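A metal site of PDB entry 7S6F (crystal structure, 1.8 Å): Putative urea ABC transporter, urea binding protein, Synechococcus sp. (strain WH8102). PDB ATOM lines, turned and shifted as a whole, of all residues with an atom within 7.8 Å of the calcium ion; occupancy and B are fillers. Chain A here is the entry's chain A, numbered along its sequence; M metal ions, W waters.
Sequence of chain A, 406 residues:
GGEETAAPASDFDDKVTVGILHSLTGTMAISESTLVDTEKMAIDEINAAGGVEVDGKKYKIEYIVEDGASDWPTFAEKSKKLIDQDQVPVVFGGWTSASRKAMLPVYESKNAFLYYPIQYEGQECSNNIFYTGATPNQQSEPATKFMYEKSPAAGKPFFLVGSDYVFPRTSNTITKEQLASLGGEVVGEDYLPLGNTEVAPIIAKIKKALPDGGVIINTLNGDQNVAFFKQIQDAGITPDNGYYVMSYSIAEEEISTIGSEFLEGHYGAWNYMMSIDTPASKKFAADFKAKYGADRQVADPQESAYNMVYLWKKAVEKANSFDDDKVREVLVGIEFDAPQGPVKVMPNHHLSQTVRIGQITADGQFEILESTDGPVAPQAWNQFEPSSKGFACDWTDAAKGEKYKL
The side-chain amide nitrogen (NE2) of Gln 353 lies within hydrogen-bond range of the side-chain amide oxygen (OE1) of Gln 138.
The side-chain carboxylate of Asp 300 lies within hydrogen-bond range of the backbone NH of Tyr 272 (2.9 Å).
The side-chain hydroxyl (OG) of Ser 304 lies close to the backbone carbonyl oxygen (O) of Asp 300.
N of Asn 271 lies within hydrogen-bond range of OD2 of Asp 300 (2.8 Å).
The backbone NH (N) of Gly 133 lies close to the backbone carbonyl oxygen (O) of Pro 117 (3.4 Å).
The side-chain hydroxyl (OG) of Ser 304 sits close to the backbone carbonyl oxygen (O) of Pro 117 (3.4 Å).
OE1 of Gln 353 sits close to NE2 of Gln 340 (3.0 Å).
The backbone NH (N) of Thr 132 lies within hydrogen-bond range of the backbone carbonyl oxygen (O) of Tyr 116, 3.1 Å away.
Merely in contact with the calcium ion: Asp 300 and Gly 133.
Within 4 Å of the calcium ion: Thr 132, Gly 133, Asp 300, Ser 304 and Gln 353.
Water W3 lies within hydrogen-bond range of the side-chain amide oxygen (OD1) of Asn 271 (2.7 Å), the side-chain carboxylate (OD1) of Asp 300 (2.8 Å) and the backbone NH (N) of Ala 134 (3.0 Å).
Water W1 lies within hydrogen-bond range of the side-chain amide nitrogen (ND2) of Asn 307 (2.9 Å), the side-chain carboxylate (OE2) of Glu 303 (2.9 Å) and the side-chain amide nitrogen (NE2) of Gln 340 (3.4 Å).
Water W2 lies within hydrogen-bond range of OE2 of Glu 303, OD2 of Asp 300 and NE2 of Gln 340.
The calcium ion is bound by the backbone carbonyl oxygen of Thr 132, the side-chain amide oxygen of Gln 353, the side-chain hydroxyl of Ser 304, water W3, water W2 and water W1.
The calcium ion has six donor atoms within binding distance.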
ATOM      1  N   TYR A 116     -17.475  11.829   0.058  1.00  0.00           N
ATOM      2  CA  TYR A 116     -16.367  11.058   0.702  1.00  0.00           C
ATOM      3  C   TYR A 116     -16.302   9.682   0.059  1.00  0.00           C
ATOM      4  O   TYR A 116     -17.315   8.984   0.045  1.00  0.00           O
ATOM      5  CB  TYR A 116     -16.647  10.980   2.200  1.00  0.00           C
ATOM      6  CG  TYR A 116     -15.752  10.042   2.970  1.00  0.00           C
ATOM      7  CD1 TYR A 116     -14.434  10.365   3.250  1.00  0.00           C
ATOM      8  CD2 TYR A 116     -16.240   8.840   3.437  1.00  0.00           C
ATOM      9  CE1 TYR A 116     -13.617   9.514   3.969  1.00  0.00           C
ATOM     10  CE2 TYR A 116     -15.434   7.980   4.154  1.00  0.00           C
ATOM     11  CZ  TYR A 116     -14.133   8.333   4.447  1.00  0.00           C
ATOM     12  OH  TYR A 116     -13.332   7.491   5.153  1.00  0.00           O
ATOM     13  N   PRO A 117     -15.149   9.263  -0.521  1.00  0.00           N
ATOM     14  CA  PRO A 117     -15.108   8.027  -1.293  1.00  0.00           C
ATOM     15  C   PRO A 117     -14.551   6.775  -0.618  1.00  0.00           C
ATOM     16  O   PRO A 117     -14.505   5.784  -1.269  1.00  0.00           O
ATOM     17  CB  PRO A 117     -14.160   8.422  -2.439  1.00  0.00           C
ATOM     18  CG  PRO A 117     -13.146   9.296  -1.761  1.00  0.00           C
ATOM     19  CD  PRO A 117     -13.925  10.060  -0.699  1.00  0.00           C
ATOM     20  N   ILE A 118     -14.117   6.852   0.634  1.00  0.00           N
ATOM     21  CA  ILE A 118     -13.230   5.784   1.156  1.00  0.00           C
ATOM     22  C   ILE A 118     -14.043   4.776   1.988  1.00  0.00           C
ATOM     23  O   ILE A 118     -14.950   5.196   2.725  1.00  0.00           O
ATOM     24  CB  ILE A 118     -12.013   6.383   1.855  1.00  0.00           C
ATOM     25  CG1 ILE A 118     -11.200   7.251   0.877  1.00  0.00           C
ATOM     26  CG2 ILE A 118     -11.201   5.272   2.482  1.00  0.00           C
ATOM     27  CD1 ILE A 118     -10.916   6.573  -0.470  1.00  0.00           C
ATOM     28  N   GLN A 119     -13.718   3.497   1.814  1.00  0.00           N
ATOM     29  CA  GLN A 119     -14.180   2.398   2.704  1.00  0.00           C
ATOM     30  C   GLN A 119     -14.045   2.854   4.161  1.00  0.00           C
ATOM     31  O   GLN A 119     -13.000   3.435   4.539  1.00  0.00           O
ATOM     32  CB  GLN A 119     -13.382   1.129   2.422  1.00  0.00           C
ATOM     33  CG  GLN A 119     -11.860   1.262   2.626  1.00  0.00           C
ATOM     34  CD  GLN A 119     -11.305   1.302   4.040  1.00  0.00           C
ATOM     35  OE1 GLN A 119     -10.313   1.954   4.321  1.00  0.00           O
ATOM     36  NE2 GLN A 119     -11.890   0.531   4.955  1.00  0.00           N
ATOM     37  N   TYR A 131     -21.439   9.130   0.530  1.00  0.00           N
ATOM     38  CA  TYR A 131     -20.395   8.089   0.666  1.00  0.00           C
ATOM     39  C   TYR A 131     -20.435   7.157  -0.546  1.00  0.00           C
ATOM     40  O   TYR A 131     -21.522   6.630  -0.861  1.00  0.00           O
ATOM     41  CB  TYR A 131     -20.684   7.297   1.939  1.00  0.00           C
ATOM     42  CG  TYR A 131     -20.953   8.110   3.174  1.00  0.00           C
ATOM     43  CD1 TYR A 131     -22.186   8.726   3.385  1.00  0.00           C
ATOM     44  CD2 TYR A 131     -20.013   8.226   4.186  1.00  0.00           C
ATOM     45  CE1 TYR A 131     -22.464   9.412   4.560  1.00  0.00           C
ATOM     46  CE2 TYR A 131     -20.287   8.885   5.368  1.00  0.00           C
ATOM     47  CZ  TYR A 131     -21.522   9.493   5.574  1.00  0.00           C
ATOM     48  OH  TYR A 131     -21.756  10.193   6.752  1.00  0.00           O
ATOM     49  N   THR A 132     -19.285   6.888  -1.172  1.00  0.00           N
ATOM     50  CA  THR A 132     -19.145   5.848  -2.215  1.00  0.00           C
ATOM     51  C   THR A 132     -18.227   4.724  -1.728  1.00  0.00           C
ATOM     52  O   THR A 132     -18.106   3.774  -2.461  1.00  0.00           O
ATOM     53  CB  THR A 132     -18.660   6.415  -3.558  1.00  0.00           C
ATOM     54  OG1 THR A 132     -17.445   7.122  -3.389  1.00  0.00           O
ATOM     55  CG2 THR A 132     -19.701   7.332  -4.154  1.00  0.00           C
ATOM     56  N   GLY A 133     -17.651   4.816  -0.552  1.00  0.00           N
ATOM     57  CA  GLY A 133     -16.788   3.742  -0.011  1.00  0.00           C
ATOM     58  C   GLY A 133     -17.662   2.679   0.664  1.00  0.00           C
ATOM     59  O   GLY A 133     -18.764   3.015   1.148  1.00  0.00           O
ATOM     60  N   ALA A 134     -17.188   1.445   0.703  1.00  0.00           N
ATOM     61  CA  ALA A 134     -17.826   0.301   1.367  1.00  0.00           C
ATOM     62  C   ALA A 134     -18.148   0.673   2.807  1.00  0.00           C
ATOM     63  O   ALA A 134     -17.299   1.180   3.520  1.00  0.00           O
ATOM     64  CB  ALA A 134     -16.908  -0.896   1.363  1.00  0.00           C
ATOM     65  N   THR A 135     -19.319   0.292   3.262  1.00  0.00           N
ATOM     66  CA  THR A 135     -19.584   0.069   4.704  1.00  0.00           C
ATOM     67  C   THR A 135     -19.076  -1.317   5.084  1.00  0.00           C
ATOM     68  O   THR A 135     -18.883  -2.188   4.244  1.00  0.00           O
ATOM     69  CB  THR A 135     -21.082   0.225   4.963  1.00  0.00           C
ATOM     70  OG1 THR A 135     -21.725  -0.670   4.052  1.00  0.00           O
ATOM     71  CG2 THR A 135     -21.539   1.637   4.713  1.00  0.00           C
ATOM     72  N   GLN A 138     -20.309  -4.365   3.244  1.00  0.00           N
ATOM     73  CA  GLN A 138     -19.790  -4.404   1.846  1.00  0.00           C
ATOM     74  C   GLN A 138     -18.273  -4.670   1.812  1.00  0.00           C
ATOM     75  O   GLN A 138     -17.714  -4.545   0.719  1.00  0.00           O
ATOM     76  CB  GLN A 138     -20.069  -3.075   1.174  1.00  0.00           C
ATOM     77  CG  GLN A 138     -21.522  -2.684   1.082  1.00  0.00           C
ATOM     78  CD  GLN A 138     -21.753  -1.309   0.479  1.00  0.00           C
ATOM     79  OE1 GLN A 138     -21.056  -0.316   0.754  1.00  0.00           O
ATOM     80  NE2 GLN A 138     -22.821  -1.221  -0.293  1.00  0.00           N
ATOM     81  N   TRP A 270     -12.945  -5.614  -1.525  1.00  0.00           N
ATOM     82  CA  TRP A 270     -13.227  -4.326  -2.184  1.00  0.00           C
ATOM     83  C   TRP A 270     -14.458  -4.495  -3.066  1.00  0.00           C
ATOM     84  O   TRP A 270     -14.919  -5.622  -3.249  1.00  0.00           O
ATOM     85  CB  TRP A 270     -12.010  -3.885  -3.006  1.00  0.00           C
ATOM     86  CG  TRP A 270     -10.809  -3.543  -2.182  1.00  0.00           C
ATOM     87  CD1 TRP A 270      -9.670  -4.269  -2.046  1.00  0.00           C
ATOM     88  CD2 TRP A 270     -10.624  -2.343  -1.416  1.00  0.00           C
ATOM     89  NE1 TRP A 270      -8.796  -3.614  -1.230  1.00  0.00           N
ATOM     90  CE2 TRP A 270      -9.357  -2.441  -0.821  1.00  0.00           C
ATOM     91  CE3 TRP A 270     -11.403  -1.214  -1.177  1.00  0.00           C
ATOM     92  CZ2 TRP A 270      -8.846  -1.435  -0.012  1.00  0.00           C
ATOM     93  CZ3 TRP A 270     -10.922  -0.227  -0.367  1.00  0.00           C
ATOM     94  CH2 TRP A 270      -9.631  -0.326   0.180  1.00  0.00           C
ATOM     95  N   ASN A 271     -14.977  -3.380  -3.579  1.00  0.00           N
ATOM     96  CA  ASN A 271     -16.131  -3.385  -4.495  1.00  0.00           C
ATOM     97  C   ASN A 271     -15.580  -3.335  -5.940  1.00  0.00           C
ATOM     98  O   ASN A 271     -16.122  -4.048  -6.796  1.00  0.00           O
ATOM     99  CB  ASN A 271     -17.077  -2.257  -4.111  1.00  0.00           C
ATOM    100  CG  ASN A 271     -17.353  -2.317  -2.627  1.00  0.00           C
ATOM    101  OD1 ASN A 271     -16.951  -1.440  -1.862  1.00  0.00           O
ATOM    102  ND2 ASN A 271     -17.992  -3.403  -2.201  1.00  0.00           N
ATOM    103  N   TYR A 272     -14.521  -2.578  -6.183  1.00  0.00           N
ATOM    104  CA  TYR A 272     -13.804  -2.564  -7.485  1.00  0.00           C
ATOM    105  C   TYR A 272     -12.404  -3.160  -7.332  1.00  0.00           C
ATOM    106  O   TYR A 272     -11.695  -2.875  -6.370  1.00  0.00           O
ATOM    107  CB  TYR A 272     -13.681  -1.169  -8.089  1.00  0.00           C
ATOM    108  CG  TYR A 272     -12.923  -1.181  -9.399  1.00  0.00           C
ATOM    109  CD1 TYR A 272     -13.508  -1.638 -10.554  1.00  0.00           C
ATOM    110  CD2 TYR A 272     -11.570  -0.822  -9.460  1.00  0.00           C
ATOM    111  CE1 TYR A 272     -12.831  -1.698 -11.747  1.00  0.00           C
ATOM    112  CE2 TYR A 272     -10.887  -0.832 -10.662  1.00  0.00           C
ATOM    113  CZ  TYR A 272     -11.500  -1.312 -11.807  1.00  0.00           C
ATOM    114  OH  TYR A 272     -10.862  -1.367 -13.017  1.00  0.00           O
ATOM    115  N   ASP A 300     -10.029   0.402  -5.929  1.00  0.00           N
ATOM    116  CA  ASP A 300     -11.351   0.746  -5.347  1.00  0.00           C
ATOM    117  C   ASP A 300     -11.426   2.209  -4.909  1.00  0.00           C
ATOM    118  O   ASP A 300     -12.398   2.921  -5.248  1.00  0.00           O
ATOM    119  CB  ASP A 300     -11.651  -0.227  -4.228  1.00  0.00           C
ATOM    120  CG  ASP A 300     -13.018   0.019  -3.661  1.00  0.00           C
ATOM    121  OD1 ASP A 300     -13.174   1.061  -3.006  1.00  0.00           O
ATOM    122  OD2 ASP A 300     -13.904  -0.770  -3.957  1.00  0.00           O
ATOM    123  N   PRO A 301     -10.443   2.738  -4.152  1.00  0.00           N
ATOM    124  CA  PRO A 301     -10.473   4.126  -3.716  1.00  0.00           C
ATOM    125  C   PRO A 301     -10.623   5.090  -4.910  1.00  0.00           C
ATOM    126  O   PRO A 301     -11.474   5.966  -4.905  1.00  0.00           O
ATOM    127  CB  PRO A 301      -9.139   4.309  -2.981  1.00  0.00           C
ATOM    128  CG  PRO A 301      -8.801   2.929  -2.513  1.00  0.00           C
ATOM    129  CD  PRO A 301      -9.235   2.040  -3.656  1.00  0.00           C
ATOM    130  N   GLN A 302      -9.879   4.819  -5.985  1.00  0.00           N
ATOM    131  CA  GLN A 302      -9.966   5.626  -7.226  1.00  0.00           C
ATOM    132  C   GLN A 302     -11.329   5.446  -7.872  1.00  0.00           C
ATOM    133  O   GLN A 302     -11.905   6.464  -8.270  1.00  0.00           O
ATOM    134  CB  GLN A 302      -8.834   5.257  -8.176  1.00  0.00           C
ATOM    135  CG  GLN A 302      -7.473   5.679  -7.644  1.00  0.00           C
ATOM    136  CD  GLN A 302      -6.417   5.017  -8.490  1.00  0.00           C
ATOM    137  OE1 GLN A 302      -6.152   5.409  -9.646  1.00  0.00           O
ATOM    138  NE2 GLN A 302      -5.854   3.976  -7.914  1.00  0.00           N
ATOM    139  N   GLU A 303     -11.806   4.207  -8.054  1.00  0.00           N
ATOM    140  CA  GLU A 303     -13.144   3.949  -8.646  1.00  0.00           C
ATOM    141  C   GLU A 303     -14.224   4.651  -7.803  1.00  0.00           C
ATOM    142  O   GLU A 303     -15.127   5.307  -8.404  1.00  0.00           O
ATOM    143  CB  GLU A 303     -13.393   2.455  -8.767  1.00  0.00           C
ATOM    144  CG  GLU A 303     -14.564   2.094  -9.653  1.00  0.00           C
ATOM    145  CD  GLU A 303     -15.871   1.806  -8.961  1.00  0.00           C
ATOM    146  OE1 GLU A 303     -16.856   1.564  -9.718  1.00  0.00           O
ATOM    147  OE2 GLU A 303     -15.920   1.837  -7.680  1.00  0.00           O
ATOM    148  N   SER A 304     -14.130   4.575  -6.474  1.00  0.00           N
ATOM    149  CA  SER A 304     -15.072   5.295  -5.580  1.00  0.00           C
ATOM    150  C   SER A 304     -15.069   6.794  -5.885  1.00  0.00           C
ATOM    151  O   SER A 304     -16.188   7.428  -5.898  1.00  0.00           O
ATOM    152  CB  SER A 304     -14.784   5.032  -4.134  1.00  0.00           C
ATOM    153  OG  SER A 304     -14.852   3.661  -3.874  1.00  0.00           O
ATOM    154  N   ALA A 305     -13.879   7.365  -6.035  1.00  0.00           N
ATOM    155  CA  ALA A 305     -13.699   8.830  -6.249  1.00  0.00           C
ATOM    156  C   ALA A 305     -14.241   9.232  -7.615  1.00  0.00           C
ATOM    157  O   ALA A 305     -14.949  10.270  -7.747  1.00  0.00           O
ATOM    158  CB  ALA A 305     -12.263   9.210  -6.072  1.00  0.00           C
ATOM    159  N   ASN A 307     -16.624   7.691  -9.378  1.00  0.00           N
ATOM    160  CA  ASN A 307     -18.102   7.581  -9.338  1.00  0.00           C
ATOM    161  C   ASN A 307     -18.721   8.822  -8.690  1.00  0.00           C
ATOM    162  O   ASN A 307     -19.798   9.267  -9.182  1.00  0.00           O
ATOM    163  CB  ASN A 307     -18.529   6.364  -8.559  1.00  0.00           C
ATOM    164  CG  ASN A 307     -18.178   5.096  -9.284  1.00  0.00           C
ATOM    165  OD1 ASN A 307     -17.867   5.118 -10.469  1.00  0.00           O
ATOM    166  ND2 ASN A 307     -18.331   3.991  -8.591  1.00  0.00           N
ATOM    167  N   GLN A 340     -17.017  -0.832 -11.672  1.00  0.00           N
ATOM    168  CA  GLN A 340     -17.237  -2.056 -10.861  1.00  0.00           C
ATOM    169  C   GLN A 340     -18.497  -2.795 -11.303  1.00  0.00           C
ATOM    170  O   GLN A 340     -18.704  -3.933 -10.856  1.00  0.00           O
ATOM    171  CB  GLN A 340     -17.355  -1.710  -9.374  1.00  0.00           C
ATOM    172  CG  GLN A 340     -18.615  -0.923  -9.025  1.00  0.00           C
ATOM    173  CD  GLN A 340     -18.950  -0.956  -7.550  1.00  0.00           C
ATOM    174  OE1 GLN A 340     -19.739  -1.771  -7.070  1.00  0.00           O
ATOM    175  NE2 GLN A 340     -18.282  -0.097  -6.796  1.00  0.00           N
ATOM    176  N   VAL A 343     -24.117   0.798  -9.752  1.00  0.00           N
ATOM    177  CA  VAL A 343     -24.137   1.403  -8.399  1.00  0.00           C
ATOM    178  C   VAL A 343     -25.354   2.331  -8.307  1.00  0.00           C
ATOM    179  O   VAL A 343     -25.783   2.881  -9.296  1.00  0.00           O
ATOM    180  CB  VAL A 343     -22.821   2.116  -8.034  1.00  0.00           C
ATOM    181  CG1 VAL A 343     -21.638   1.153  -8.134  1.00  0.00           C
ATOM    182  CG2 VAL A 343     -22.571   3.351  -8.875  1.00  0.00           C
ATOM    183  N   LEU A 351     -23.763   3.852  -1.019  1.00  0.00           N
ATOM    184  CA  LEU A 351     -23.814   3.323  -2.407  1.00  0.00           C
ATOM    185  C   LEU A 351     -24.001   1.818  -2.375  1.00  0.00           C
ATOM    186  O   LEU A 351     -23.203   1.148  -1.713  1.00  0.00           O
ATOM    187  CB  LEU A 351     -22.511   3.737  -3.097  1.00  0.00           C
ATOM    188  CG  LEU A 351     -22.525   3.650  -4.620  1.00  0.00           C
ATOM    189  CD1 LEU A 351     -23.417   4.701  -5.236  1.00  0.00           C
ATOM    190  CD2 LEU A 351     -21.110   3.762  -5.165  1.00  0.00           C
ATOM    191  N   SER A 352     -25.035   1.296  -3.043  1.00  0.00           N
ATOM    192  CA  SER A 352     -25.181  -0.153  -3.305  1.00  0.00           C
ATOM    193  C   SER A 352     -24.112  -0.551  -4.308  1.00  0.00           C
ATOM    194  O   SER A 352     -23.944   0.150  -5.324  1.00  0.00           O
ATOM    195  CB  SER A 352     -26.590  -0.594  -3.742  1.00  0.00           C
ATOM    196  OG  SER A 352     -26.830  -0.151  -5.024  1.00  0.00           O
ATOM    197  N   GLN A 353     -23.340  -1.569  -3.932  1.00  0.00           N
ATOM    198  CA  GLN A 353     -22.086  -1.977  -4.609  1.00  0.00           C
ATOM    199  C   GLN A 353     -21.927  -3.500  -4.549  1.00  0.00           C
ATOM    200  O   GLN A 353     -22.411  -4.141  -3.586  1.00  0.00           O
ATOM    201  CB  GLN A 353     -20.877  -1.370  -3.901  1.00  0.00           C
ATOM    202  CG  GLN A 353     -20.929   0.137  -3.857  1.00  0.00           C
ATOM    203  CD  GLN A 353     -19.669   0.707  -3.267  1.00  0.00           C
ATOM    204  OE1 GLN A 353     -18.701   0.882  -3.982  1.00  0.00           O
ATOM    205  NE2 GLN A 353     -19.702   1.083  -1.997  1.00  0.00           N
ATOM    206  N   THR A 354     -21.178  -4.042  -5.502  1.00  0.00           N
ATOM    207  CA  THR A 354     -20.894  -5.487  -5.608  1.00  0.00           C
ATOM    208  C   THR A 354     -19.699  -5.750  -4.697  1.00  0.00           C
ATOM    209  O   THR A 354     -18.887  -4.868  -4.575  1.00  0.00           O
ATOM    210  CB  THR A 354     -20.662  -5.849  -7.079  1.00  0.00           C
ATOM    211  OG1 THR A 354     -21.883  -5.597  -7.787  1.00  0.00           O
ATOM    212  CG2 THR A 354     -20.253  -7.293  -7.250  1.00  0.00           C
HETATM  213 CA    CA M   1     -16.799   2.265  -3.649  1.00  0.00          CA
HETATM  214  O   HOH W   1     -17.833   3.123  -5.848  1.00  0.00           O
HETATM  215  O   HOH W   2     -15.651   0.881  -5.303  1.00  0.00           O
HETATM  216  O   HOH W   3     -15.750   0.983  -1.885  1.00  0.00           O
